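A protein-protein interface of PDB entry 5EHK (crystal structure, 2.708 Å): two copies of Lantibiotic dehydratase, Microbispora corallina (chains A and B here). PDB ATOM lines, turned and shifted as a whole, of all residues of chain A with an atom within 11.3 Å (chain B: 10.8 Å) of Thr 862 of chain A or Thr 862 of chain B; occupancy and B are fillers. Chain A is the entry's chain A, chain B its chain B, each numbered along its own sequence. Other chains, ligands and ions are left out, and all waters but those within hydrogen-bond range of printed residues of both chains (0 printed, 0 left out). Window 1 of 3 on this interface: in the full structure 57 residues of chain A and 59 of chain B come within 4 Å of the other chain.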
ATOM      1  N   ARG A 408      -8.090  14.833  15.253  1.00  0.00           N
ATOM      2  CA  ARG A 408      -7.647  13.454  15.426  1.00  0.00           C
ATOM      3  C   ARG A 408      -8.633  12.654  16.294  1.00  0.00           C
ATOM      4  O   ARG A 408      -8.832  11.466  16.075  1.00  0.00           O
ATOM      5  CB  ARG A 408      -6.223  13.390  15.989  1.00  0.00           C
ATOM      6  CG  ARG A 408      -5.140  13.974  15.059  1.00  0.00           C
ATOM      7  CD  ARG A 408      -3.795  14.096  15.803  1.00  0.00           C
ATOM      8  NE  ARG A 408      -3.346  12.755  16.187  1.00  0.00           N
ATOM      9  CZ  ARG A 408      -2.753  11.902  15.354  1.00  0.00           C
ATOM     10  NH1 ARG A 408      -2.472  12.278  14.110  1.00  0.00           N
ATOM     11  NH2 ARG A 408      -2.424  10.689  15.769  1.00  0.00           N
ATOM     12  N   ALA A 412     -10.451   9.170  15.481  1.00  0.00           N
ATOM     13  CA  ALA A 412     -10.361   8.071  16.419  1.00  0.00           C
ATOM     14  C   ALA A 412     -11.769   7.529  16.680  1.00  0.00           C
ATOM     15  O   ALA A 412     -12.007   6.310  16.611  1.00  0.00           O
ATOM     16  CB  ALA A 412      -9.700   8.541  17.701  1.00  0.00           C
ATOM     17  N   GLU A 415     -13.200   5.549  13.965  1.00  0.00           N
ATOM     18  CA  GLU A 415     -12.520   4.272  13.898  1.00  0.00           C
ATOM     19  C   GLU A 415     -13.097   3.274  14.911  1.00  0.00           C
ATOM     20  O   GLU A 415     -13.324   2.105  14.593  1.00  0.00           O
ATOM     21  CB  GLU A 415     -11.006   4.491  14.107  1.00  0.00           C
ATOM     22  CG  GLU A 415     -10.153   3.242  14.267  1.00  0.00           C
ATOM     23  CD  GLU A 415      -9.659   2.704  12.923  1.00  0.00           C
ATOM     24  OE1 GLU A 415     -10.357   2.925  11.899  1.00  0.00           O
ATOM     25  OE2 GLU A 415      -8.579   2.055  12.895  1.00  0.00           O
ATOM     26  N   GLU A 447      -3.566  11.079  28.194  1.00  0.00           N
ATOM     27  CA  GLU A 447      -2.390  10.280  27.913  1.00  0.00           C
ATOM     28  C   GLU A 447      -2.173  10.071  26.399  1.00  0.00           C
ATOM     29  O   GLU A 447      -1.138   9.561  25.978  1.00  0.00           O
ATOM     30  CB  GLU A 447      -2.461   8.955  28.707  1.00  0.00           C
ATOM     31  CG  GLU A 447      -2.331   9.145  30.252  1.00  0.00           C
ATOM     32  CD  GLU A 447      -3.045   8.059  31.093  1.00  0.00           C
ATOM     33  OE1 GLU A 447      -3.503   7.038  30.506  1.00  0.00           O
ATOM     34  OE2 GLU A 447      -3.143   8.234  32.346  1.00  0.00           O
ATOM     35  N   THR A 448      -3.103  10.560  25.585  1.00  0.00           N
ATOM     36  CA  THR A 448      -3.023  10.389  24.138  1.00  0.00           C
ATOM     37  C   THR A 448      -1.983  11.317  23.530  1.00  0.00           C
ATOM     38  O   THR A 448      -1.988  12.524  23.778  1.00  0.00           O
ATOM     39  CB  THR A 448      -4.367  10.700  23.452  1.00  0.00           C
ATOM     40  OG1 THR A 448      -5.372   9.819  23.930  1.00  0.00           O
ATOM     41  CG2 THR A 448      -4.253  10.534  21.951  1.00  0.00           C
ATOM     42  N   PRO A 449      -1.089  10.762  22.707  1.00  0.00           N
ATOM     43  CA  PRO A 449      -0.060  11.630  22.117  1.00  0.00           C
ATOM     44  C   PRO A 449      -0.637  12.657  21.132  1.00  0.00           C
ATOM     45  O   PRO A 449      -1.572  12.354  20.399  1.00  0.00           O
ATOM     46  CB  PRO A 449       0.851  10.634  21.377  1.00  0.00           C
ATOM     47  CG  PRO A 449      -0.038   9.457  21.063  1.00  0.00           C
ATOM     48  CD  PRO A 449      -0.987   9.365  22.243  1.00  0.00           C
ATOM     49  N   ARG A 823      -2.450 -13.389  17.987  1.00  0.00           N
ATOM     50  CA  ARG A 823      -1.761 -12.389  17.167  1.00  0.00           C
ATOM     51  C   ARG A 823      -0.382 -12.852  16.762  1.00  0.00           C
ATOM     52  O   ARG A 823       0.491 -13.043  17.593  1.00  0.00           O
ATOM     53  CB  ARG A 823      -1.646 -11.095  17.908  1.00  0.00           C
ATOM     54  CG  ARG A 823      -2.966 -10.573  18.360  1.00  0.00           C
ATOM     55  CD  ARG A 823      -2.762  -9.145  18.800  1.00  0.00           C
ATOM     56  NE  ARG A 823      -3.920  -8.646  19.520  1.00  0.00           N
ATOM     57  CZ  ARG A 823      -3.821  -7.994  20.666  1.00  0.00           C
ATOM     58  NH1 ARG A 823      -2.610  -7.801  21.207  1.00  0.00           N
ATOM     59  NH2 ARG A 823      -4.923  -7.562  21.266  1.00  0.00           N
ATOM     60  N   ARG A 825       2.980 -12.180  14.902  1.00  0.00           N
ATOM     61  CA  ARG A 825       3.797 -11.071  14.409  1.00  0.00           C
ATOM     62  C   ARG A 825       4.633 -11.532  13.228  1.00  0.00           C
ATOM     63  O   ARG A 825       5.818 -11.719  13.331  1.00  0.00           O
ATOM     64  CB  ARG A 825       4.665 -10.482  15.525  1.00  0.00           C
ATOM     65  CG  ARG A 825       3.864  -9.992  16.734  1.00  0.00           C
ATOM     66  CD  ARG A 825       3.226  -8.636  16.496  1.00  0.00           C
ATOM     67  NE  ARG A 825       2.047  -8.390  17.333  1.00  0.00           N
ATOM     68  CZ  ARG A 825       1.284  -7.298  17.236  1.00  0.00           C
ATOM     69  NH1 ARG A 825       1.589  -6.357  16.335  1.00  0.00           N
ATOM     70  NH2 ARG A 825       0.224  -7.145  18.033  1.00  0.00           N
ATOM     71  N   TYR A 859      -4.032  -7.634   9.928  1.00  0.00           N
ATOM     72  CA  TYR A 859      -4.404  -6.551  10.811  1.00  0.00           C
ATOM     73  C   TYR A 859      -3.197  -5.646  10.975  1.00  0.00           C
ATOM     74  O   TYR A 859      -2.054  -6.100  10.920  1.00  0.00           O
ATOM     75  CB  TYR A 859      -4.836  -7.121  12.177  1.00  0.00           C
ATOM     76  CG  TYR A 859      -5.727  -6.206  12.980  1.00  0.00           C
ATOM     77  CD1 TYR A 859      -7.108  -6.383  12.978  1.00  0.00           C
ATOM     78  CD2 TYR A 859      -5.197  -5.149  13.729  1.00  0.00           C
ATOM     79  CE1 TYR A 859      -7.953  -5.542  13.702  1.00  0.00           C
ATOM     80  CE2 TYR A 859      -6.035  -4.296  14.462  1.00  0.00           C
ATOM     81  CZ  TYR A 859      -7.417  -4.502  14.442  1.00  0.00           C
ATOM     82  OH  TYR A 859      -8.273  -3.685  15.153  1.00  0.00           O
ATOM     83  N   SER A 860      -3.436  -4.366  11.196  1.00  0.00           N
ATOM     84  CA  SER A 860      -2.342  -3.486  11.571  1.00  0.00           C
ATOM     85  C   SER A 860      -2.690  -2.719  12.845  1.00  0.00           C
ATOM     86  O   SER A 860      -3.703  -2.024  12.889  1.00  0.00           O
ATOM     87  CB  SER A 860      -2.010  -2.532  10.431  1.00  0.00           C
ATOM     88  OG  SER A 860      -1.147  -1.529  10.902  1.00  0.00           O
ATOM     89  N   ASP A 861      -1.885  -2.878  13.895  1.00  0.00           N
ATOM     90  CA  ASP A 861      -2.059  -2.073  15.109  1.00  0.00           C
ATOM     91  C   ASP A 861      -0.864  -1.165  15.379  1.00  0.00           C
ATOM     92  O   ASP A 861      -0.008  -0.959  14.511  1.00  0.00           O
ATOM     93  CB  ASP A 861      -2.394  -2.939  16.344  1.00  0.00           C
ATOM     94  CG  ASP A 861      -1.305  -3.997  16.675  1.00  0.00           C
ATOM     95  OD1 ASP A 861      -0.125  -3.838  16.279  1.00  0.00           O
ATOM     96  OD2 ASP A 861      -1.630  -4.986  17.387  1.00  0.00           O
ATOM     97  N   THR A 862      -0.760  -0.695  16.613  1.00  0.00           N
ATOM     98  CA  THR A 862       0.291   0.255  16.961  1.00  0.00           C
ATOM     99  C   THR A 862       1.672  -0.392  16.811  1.00  0.00           C
ATOM    100  O   THR A 862       2.684   0.306  16.780  1.00  0.00           O
ATOM    101  CB  THR A 862       0.146   0.773  18.426  1.00  0.00           C
ATOM    102  OG1 THR A 862       0.201  -0.331  19.341  1.00  0.00           O
ATOM    103  CG2 THR A 862      -1.166   1.564  18.640  1.00  0.00           C
ATOM    104  N   ALA A 863       1.712  -1.721  16.734  1.00  0.00           N
ATOM    105  CA  ALA A 863       2.980  -2.444  16.670  1.00  0.00           C
ATOM    106  C   ALA A 863       3.268  -3.012  15.288  1.00  0.00           C
ATOM    107  O   ALA A 863       4.182  -3.825  15.106  1.00  0.00           O
ATOM    108  CB  ALA A 863       3.025  -3.542  17.719  1.00  0.00           C
ATOM    109  N   GLY A 864       2.494  -2.579  14.307  1.00  0.00           N
ATOM    110  CA  GLY A 864       2.792  -2.942  12.942  1.00  0.00           C
ATOM    111  C   GLY A 864       1.768  -3.886  12.353  1.00  0.00           C
ATOM    112  O   GLY A 864       0.660  -4.018  12.882  1.00  0.00           O
ATOM    113  N   GLN A 865       2.161  -4.533  11.253  1.00  0.00           N
ATOM    114  CA  GLN A 865       1.321  -5.483  10.537  1.00  0.00           C
ATOM    115  C   GLN A 865       1.520  -6.892  11.043  1.00  0.00           C
ATOM    116  O   GLN A 865       2.660  -7.355  11.195  1.00  0.00           O
ATOM    117  CB  GLN A 865       1.615  -5.442   9.039  1.00  0.00           C
ATOM    118  CG  GLN A 865       0.836  -4.377   8.282  1.00  0.00           C
ATOM    119  CD  GLN A 865       1.336  -4.200   6.873  1.00  0.00           C
ATOM    120  OE1 GLN A 865       2.531  -4.031   6.659  1.00  0.00           O
ATOM    121  NE2 GLN A 865       0.430  -4.243   5.896  1.00  0.00           N
ATOM    122  N   HIS A 866       0.407  -7.573  11.305  1.00  0.00           N
ATOM    123  CA  HIS A 866       0.472  -8.945  11.783  1.00  0.00           C
ATOM    124  C   HIS A 866      -0.716  -9.746  11.276  1.00  0.00           C
ATOM    125  O   HIS A 866      -1.541  -9.225  10.549  1.00  0.00           O
ATOM    126  CB  HIS A 866       0.577  -8.952  13.295  1.00  0.00           C
ATOM    127  CG  HIS A 866      -0.533  -8.222  13.967  1.00  0.00           C
ATOM    128  ND1 HIS A 866      -0.665  -6.853  13.894  1.00  0.00           N
ATOM    129  CD2 HIS A 866      -1.536  -8.657  14.766  1.00  0.00           C
ATOM    130  CE1 HIS A 866      -1.729  -6.481  14.585  1.00  0.00           C
ATOM    131  NE2 HIS A 866      -2.267  -7.555  15.137  1.00  0.00           N
ATOM    132  N   ARG A 868      -3.974 -12.182  12.465  1.00  0.00           N
ATOM    133  CA  ARG A 868      -4.755 -12.608  13.613  1.00  0.00           C
ATOM    134  C   ARG A 868      -5.504 -13.859  13.222  1.00  0.00           C
ATOM    135  O   ARG A 868      -6.180 -13.892  12.210  1.00  0.00           O
ATOM    136  CB  ARG A 868      -5.709 -11.507  14.044  1.00  0.00           C
ATOM    137  CG  ARG A 868      -4.978 -10.283  14.447  1.00  0.00           C
ATOM    138  CD  ARG A 868      -5.862  -9.327  15.144  1.00  0.00           C
ATOM    139  NE  ARG A 868      -5.062  -8.372  15.898  1.00  0.00           N
ATOM    140  CZ  ARG A 868      -5.558  -7.324  16.541  1.00  0.00           C
ATOM    141  NH1 ARG A 868      -6.867  -7.093  16.499  1.00  0.00           N
ATOM    142  NH2 ARG A 868      -4.740  -6.513  17.205  1.00  0.00           N
ATOM    143  N   GLU A 903       0.927 -13.107  20.676  1.00  0.00           N
ATOM    144  CA  GLU A 903       0.136 -12.842  21.880  1.00  0.00           C
ATOM    145  C   GLU A 903      -1.257 -13.448  21.809  1.00  0.00           C
ATOM    146  O   GLU A 903      -1.712 -13.872  20.749  1.00  0.00           O
ATOM    147  CB  GLU A 903      -0.003 -11.350  22.137  1.00  0.00           C
ATOM    148  CG  GLU A 903       1.262 -10.562  21.987  1.00  0.00           C
ATOM    149  CD  GLU A 903       1.218  -9.725  20.744  1.00  0.00           C
ATOM    150  OE1 GLU A 903       0.184  -9.035  20.524  1.00  0.00           O
ATOM    151  OE2 GLU A 903       2.204  -9.774  19.974  1.00  0.00           O
ATOM    152  N   ARG B 408      17.067   7.419  14.989  1.00  0.00           N
ATOM    153  CA  ARG B 408      16.054   6.626  15.681  1.00  0.00           C
ATOM    154  C   ARG B 408      16.476   5.152  15.668  1.00  0.00           C
ATOM    155  O   ARG B 408      16.301   4.452  16.661  1.00  0.00           O
ATOM    156  CB  ARG B 408      14.659   6.840  15.078  1.00  0.00           C
ATOM    157  CG  ARG B 408      14.153   8.257  15.311  1.00  0.00           C
ATOM    158  CD  ARG B 408      12.958   8.604  14.418  1.00  0.00           C
ATOM    159  NE  ARG B 408      11.799   7.745  14.655  1.00  0.00           N
ATOM    160  CZ  ARG B 408      10.972   7.870  15.690  1.00  0.00           C
ATOM    161  NH1 ARG B 408      11.185   8.800  16.615  1.00  0.00           N
ATOM    162  NH2 ARG B 408       9.950   7.036  15.815  1.00  0.00           N
ATOM    163  N   GLU B 415      17.824   0.441  22.987  1.00  0.00           N
ATOM    164  CA  GLU B 415      16.646   0.059  23.741  1.00  0.00           C
ATOM    165  C   GLU B 415      16.473  -1.475  23.718  1.00  0.00           C
ATOM    166  O   GLU B 415      16.199  -2.075  24.747  1.00  0.00           O
ATOM    167  CB  GLU B 415      15.426   0.774  23.152  1.00  0.00           C
ATOM    168  CG  GLU B 415      14.084   0.271  23.643  1.00  0.00           C
ATOM    169  CD  GLU B 415      13.629   0.975  24.894  1.00  0.00           C
ATOM    170  OE1 GLU B 415      14.511   1.409  25.673  1.00  0.00           O
ATOM    171  OE2 GLU B 415      12.394   1.101  25.091  1.00  0.00           O
ATOM    172  N   GLU B 447       9.174  -1.354   7.095  1.00  0.00           N
ATOM    173  CA  GLU B 447       7.823  -1.193   7.604  1.00  0.00           C
ATOM    174  C   GLU B 447       7.829  -0.277   8.839  1.00  0.00           C
ATOM    175  O   GLU B 447       6.784  -0.068   9.461  1.00  0.00           O
ATOM    176  CB  GLU B 447       7.219  -2.571   7.906  1.00  0.00           C
ATOM    177  CG  GLU B 447       6.968  -3.454   6.648  1.00  0.00           C
ATOM    178  CD  GLU B 447       7.032  -4.968   6.945  1.00  0.00           C
ATOM    179  OE1 GLU B 447       7.106  -5.331   8.149  1.00  0.00           O
ATOM    180  OE2 GLU B 447       6.991  -5.793   5.985  1.00  0.00           O
ATOM    181  N   THR B 448       9.012   0.228   9.219  1.00  0.00           N
ATOM    182  CA  THR B 448       9.130   1.117  10.379  1.00  0.00           C
ATOM    183  C   THR B 448       8.644   2.530  10.034  1.00  0.00           C
ATOM    184  O   THR B 448       9.035   3.123   9.015  1.00  0.00           O
ATOM    185  CB  THR B 448      10.580   1.163  10.973  1.00  0.00           C
ATOM    186  OG1 THR B 448      10.934  -0.112  11.502  1.00  0.00           O
ATOM    187  CG2 THR B 448      10.680   2.146  12.105  1.00  0.00           C
ATOM    188  N   PRO B 449       7.765   3.075  10.881  1.00  0.00           N
ATOM    189  CA  PRO B 449       7.270   4.422  10.591  1.00  0.00           C
ATOM    190  C   PRO B 449       8.399   5.444  10.727  1.00  0.00           C
ATOM    191  O   PRO B 449       9.252   5.276  11.607  1.00  0.00           O
ATOM    192  CB  PRO B 449       6.186   4.633  11.662  1.00  0.00           C
ATOM    193  CG  PRO B 449       6.577   3.727  12.791  1.00  0.00           C
ATOM    194  CD  PRO B 449       7.200   2.521  12.125  1.00  0.00           C
ATOM    195  N   ARG B 823      -0.838  -8.782  30.225  1.00  0.00           N
ATOM    196  CA  ARG B 823      -0.822  -7.342  30.018  1.00  0.00           C
ATOM    197  C   ARG B 823      -2.208  -6.809  30.338  1.00  0.00           C
ATOM    198  O   ARG B 823      -3.173  -7.164  29.672  1.00  0.00           O
ATOM    199  CB  ARG B 823      -0.502  -7.014  28.591  1.00  0.00           C
ATOM    200  CG  ARG B 823       0.741  -7.675  28.141  1.00  0.00           C
ATOM    201  CD  ARG B 823       1.228  -7.044  26.878  1.00  0.00           C
ATOM    202  NE  ARG B 823       2.298  -7.821  26.280  1.00  0.00           N
ATOM    203  CZ  ARG B 823       2.369  -8.057  24.986  1.00  0.00           C
ATOM    204  NH1 ARG B 823       1.426  -7.544  24.179  1.00  0.00           N
ATOM    205  NH2 ARG B 823       3.382  -8.772  24.512  1.00  0.00           N
ATOM    206  N   ARG B 825      -4.565  -3.638  30.593  1.00  0.00           N
ATOM    207  CA  ARG B 825      -4.671  -2.258  30.078  1.00  0.00           C
ATOM    208  C   ARG B 825      -5.369  -1.347  31.054  1.00  0.00           C
ATOM    209  O   ARG B 825      -6.497  -0.941  30.830  1.00  0.00           O
ATOM    210  CB  ARG B 825      -5.390  -2.216  28.728  1.00  0.00           C
ATOM    211  CG  ARG B 825      -4.713  -3.107  27.676  1.00  0.00           C
ATOM    212  CD  ARG B 825      -3.475  -2.426  27.136  1.00  0.00           C
ATOM    213  NE  ARG B 825      -2.475  -3.371  26.650  1.00  0.00           N
ATOM    214  CZ  ARG B 825      -1.270  -3.013  26.212  1.00  0.00           C
ATOM    215  NH1 ARG B 825      -0.920  -1.719  26.203  1.00  0.00           N
ATOM    216  NH2 ARG B 825      -0.421  -3.948  25.794  1.00  0.00           N
ATOM    217  N   TYR B 859       4.662  -0.727  32.557  1.00  0.00           N
ATOM    218  CA  TYR B 859       5.283  -0.790  31.234  1.00  0.00           C
ATOM    219  C   TYR B 859       4.579   0.167  30.303  1.00  0.00           C
ATOM    220  O   TYR B 859       3.397   0.472  30.470  1.00  0.00           O
ATOM    221  CB  TYR B 859       5.121  -2.200  30.657  1.00  0.00           C
ATOM    222  CG  TYR B 859       6.097  -2.615  29.573  1.00  0.00           C
ATOM    223  CD1 TYR B 859       7.173  -3.466  29.863  1.00  0.00           C
ATOM    224  CD2 TYR B 859       5.916  -2.210  28.250  1.00  0.00           C
ATOM    225  CE1 TYR B 859       8.075  -3.865  28.865  1.00  0.00           C
ATOM    226  CE2 TYR B 859       6.805  -2.598  27.244  1.00  0.00           C
ATOM    227  CZ  TYR B 859       7.882  -3.428  27.555  1.00  0.00           C
ATOM    228  OH  TYR B 859       8.759  -3.817  26.561  1.00  0.00           O
ATOM    229  N   SER B 860       5.317   0.657  29.322  1.00  0.00           N
ATOM    230  CA  SER B 860       4.698   1.375  28.226  1.00  0.00           C
ATOM    231  C   SER B 860       5.127   0.753  26.903  1.00  0.00           C
ATOM    232  O   SER B 860       6.322   0.647  26.610  1.00  0.00           O
ATOM    233  CB  SER B 860       5.067   2.843  28.240  1.00  0.00           C
ATOM    234  OG  SER B 860       4.679   3.407  26.998  1.00  0.00           O
ATOM    235  N   ASP B 861       4.155   0.307  26.119  1.00  0.00           N
ATOM    236  CA  ASP B 861       4.458  -0.179  24.779  1.00  0.00           C
ATOM    237  C   ASP B 861       3.807   0.790  23.823  1.00  0.00           C
ATOM    238  O   ASP B 861       3.540   1.934  24.181  1.00  0.00           O
ATOM    239  CB  ASP B 861       3.998  -1.644  24.559  1.00  0.00           C
ATOM    240  CG  ASP B 861       2.461  -1.847  24.682  1.00  0.00           C
ATOM    241  OD1 ASP B 861       1.659  -0.909  24.445  1.00  0.00           O
ATOM    242  OD2 ASP B 861       2.058  -2.974  25.030  1.00  0.00           O
ATOM    243  N   THR B 862       3.580   0.344  22.601  1.00  0.00           N
ATOM    244  CA  THR B 862       2.993   1.214  21.589  1.00  0.00           C
ATOM    245  C   THR B 862       1.526   1.595  21.843  1.00  0.00           C
ATOM    246  O   THR B 862       1.027   2.575  21.284  1.00  0.00           O
ATOM    247  CB  THR B 862       3.188   0.623  20.197  1.00  0.00           C
ATOM    248  OG1 THR B 862       2.727  -0.732  20.208  1.00  0.00           O
ATOM    249  CG2 THR B 862       4.654   0.624  19.846  1.00  0.00           C
ATOM    250  N   ALA B 863       0.850   0.848  22.710  1.00  0.00           N
ATOM    251  CA  ALA B 863      -0.569   1.097  22.969  1.00  0.00           C
ATOM    252  C   ALA B 863      -0.810   1.797  24.313  1.00  0.00           C
ATOM    253  O   ALA B 863      -1.939   1.846  24.819  1.00  0.00           O
ATOM    254  CB  ALA B 863      -1.380  -0.192  22.866  1.00  0.00           C
ATOM    255  N   GLY B 864       0.257   2.338  24.885  1.00  0.00           N
ATOM    256  CA  GLY B 864       0.123   3.173  26.055  1.00  0.00           C
ATOM    257  C   GLY B 864       0.724   2.583  27.304  1.00  0.00           C
ATOM    258  O   GLY B 864       1.566   1.680  27.240  1.00  0.00           O
ATOM    259  N   GLN B 865       0.314   3.127  28.445  1.00  0.00           N
ATOM    260  CA  GLN B 865       0.793   2.651  29.737  1.00  0.00           C
ATOM    261  C   GLN B 865      -0.101   1.562  30.289  1.00  0.00           C
ATOM    262  O   GLN B 865      -1.324   1.705  30.296  1.00  0.00           O
ATOM    263  CB  GLN B 865       0.960   3.805  30.737  1.00  0.00           C
ATOM    264  CG  GLN B 865       2.353   4.464  30.680  1.00  0.00           C
ATOM    265  CD  GLN B 865       2.436   5.760  31.470  1.00  0.00           C
ATOM    266  OE1 GLN B 865       1.624   6.661  31.284  1.00  0.00           O
ATOM    267  NE2 GLN B 865       3.406   5.843  32.386  1.00  0.00           N
ATOM    268  N   HIS B 866       0.518   0.465  30.723  1.00  0.00           N
ATOM    269  CA  HIS B 866      -0.230  -0.660  31.259  1.00  0.00           C
ATOM    270  C   HIS B 866       0.568  -1.364  32.334  1.00  0.00           C
ATOM    271  O   HIS B 866       1.700  -0.980  32.629  1.00  0.00           O
ATOM    272  CB  HIS B 866      -0.602  -1.655  30.150  1.00  0.00           C
ATOM    273  CG  HIS B 866       0.583  -2.165  29.397  1.00  0.00           C
ATOM    274  ND1 HIS B 866       1.266  -1.395  28.482  1.00  0.00           N
ATOM    275  CD2 HIS B 866       1.255  -3.337  29.481  1.00  0.00           C
ATOM    276  CE1 HIS B 866       2.296  -2.079  28.017  1.00  0.00           C
ATOM    277  NE2 HIS B 866       2.313  -3.258  28.611  1.00  0.00           N
ATOM    278  N   ARG B 868       2.047  -5.156  33.678  1.00  0.00           N
ATOM    279  CA  ARG B 868       2.316  -6.514  33.273  1.00  0.00           C
ATOM    280  C   ARG B 868       2.449  -7.310  34.527  1.00  0.00           C
ATOM    281  O   ARG B 868       3.165  -6.909  35.418  1.00  0.00           O
ATOM    282  CB  ARG B 868       3.573  -6.608  32.417  1.00  0.00           C
ATOM    283  CG  ARG B 868       3.446  -5.818  31.168  1.00  0.00           C
ATOM    284  CD  ARG B 868       4.495  -6.160  30.190  1.00  0.00           C
ATOM    285  NE  ARG B 868       4.099  -5.708  28.862  1.00  0.00           N
ATOM    286  CZ  ARG B 868       4.869  -5.779  27.785  1.00  0.00           C
ATOM    287  NH1 ARG B 868       6.085  -6.301  27.868  1.00  0.00           N
ATOM    288  NH2 ARG B 868       4.413  -5.333  26.622  1.00  0.00           N
ATOM    289  N   GLU B 903      -4.125  -8.892  27.442  1.00  0.00           N
ATOM    290  CA  GLU B 903      -3.522  -9.872  26.546  1.00  0.00           C
ATOM    291  C   GLU B 903      -2.598 -10.814  27.304  1.00  0.00           C
ATOM    292  O   GLU B 903      -2.185 -10.542  28.432  1.00  0.00           O
ATOM    293  CB  GLU B 903      -2.738  -9.245  25.395  1.00  0.00           C
ATOM    294  CG  GLU B 903      -3.430  -8.144  24.657  1.00  0.00           C
ATOM    295  CD  GLU B 903      -2.797  -6.808  24.968  1.00  0.00           C
ATOM    296  OE1 GLU B 903      -1.568  -6.654  24.748  1.00  0.00           O
ATOM    297  OE2 GLU B 903      -3.529  -5.920  25.457  1.00  0.00           O
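N of Ala 863 of chain B is in hydrogen-bond range of OD1 of Asp 861 of chain B, at 2.6 Å. The side-chain carboxylate (OE1) of Glu 903 of chain A lies within salt-bridge range of the guanidinium group (NH1) of Arg 823 of chain A (3.1 Å). The guanidinium group (NE) of Arg 825 of chain A lies within salt-bridge range of the side-chain carboxylate (OE2) of Glu 903 of chain A (3.0 Å). The side-chain carboxylate (OE2) of Glu 903 of chain B lies within salt-bridge range of the guanidinium group (NE) of Arg 825 of chain B, 3.0 Å away. N of Ala 863 of chain A is in hydrogen-bond range of OD1 of Asp 861 of chain A, at 2.8 Å. The guanidinium group of Arg 823 of chain B is in salt-bridge range of the side-chain carboxylate of Glu 903 of chain B (3.2 Å).
Arg 823 of chain A touches Glu 903 of chain B, and with the chains exchanged Glu 903 of chain A touches Arg 823 of chain B. Thr 862 of chain A touches its own counterpart, Thr 862 of chain B. Thr 862 of chain A touches Ala 863 of chain B, and with the chains exchanged Ala 863 of chain A touches Thr 862 of chain B. Of the 5 pairs that touch across the chains among the printed residues, 5 have their exchanged pair printed and touching as well.
Thr 862 of chain A touches Ala 863 of chain B. Thr 862 of chain B touches Ala 863 of chain A (OG1 to N, 3.8 Å). Glu 903 of chain A touches Arg 823 of chain B (CG to NH1, 3.7 Å).
Hydrophobic or aromatic side chains of chain B within 4 Å of the printed part of chain A: Ala 863. Among the printed residues, 5 pairs touch across the chains. Among the printed residues, Asp or Glu carboxylates within 4 Å of a Lys or Arg side-chain nitrogen of the other chain: Arg 823 of chain A with Glu 903 of chain B (3.9 Å).
Printed residues of chain B within 4 Å of Arg 823 of chain A: Glu 903. Ala 863 of chain A touches one residue of chain B. Of the printed residues of chain B, Glu 903 of chain A touches Arg 823. Of the printed residues of chain A, Arg 823 of chain B touches Glu 903 (3.7 Å). No residue of chain A comes within 4 Å of Ser 860 of chain B. No residue of chain A comes within 4 Å of Asp 861 of chain B. Thr 862 of chain B touches two residues of chain A. Gly 864 of chain B touches none of the printed residues of chain A. The nearest residue of chain B that does not touch Thr 862 of chain A is Asp 861 of chain B (5.3 Å). The nearest residue of chain A that does not touch Thr 862 of chain B is Asp 861 of chain A (5.8 Å).
The side-chain hydroxyl (OG1) of Thr 862 of chain A sits at hydrogen-bond distance from the side-chain hydroxyl (OG1) of Thr 862 of chain B (2.7 Å). OE1 of Glu 903 of chain B is in salt-bridge range of NH1 of Arg 823 of chain A.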
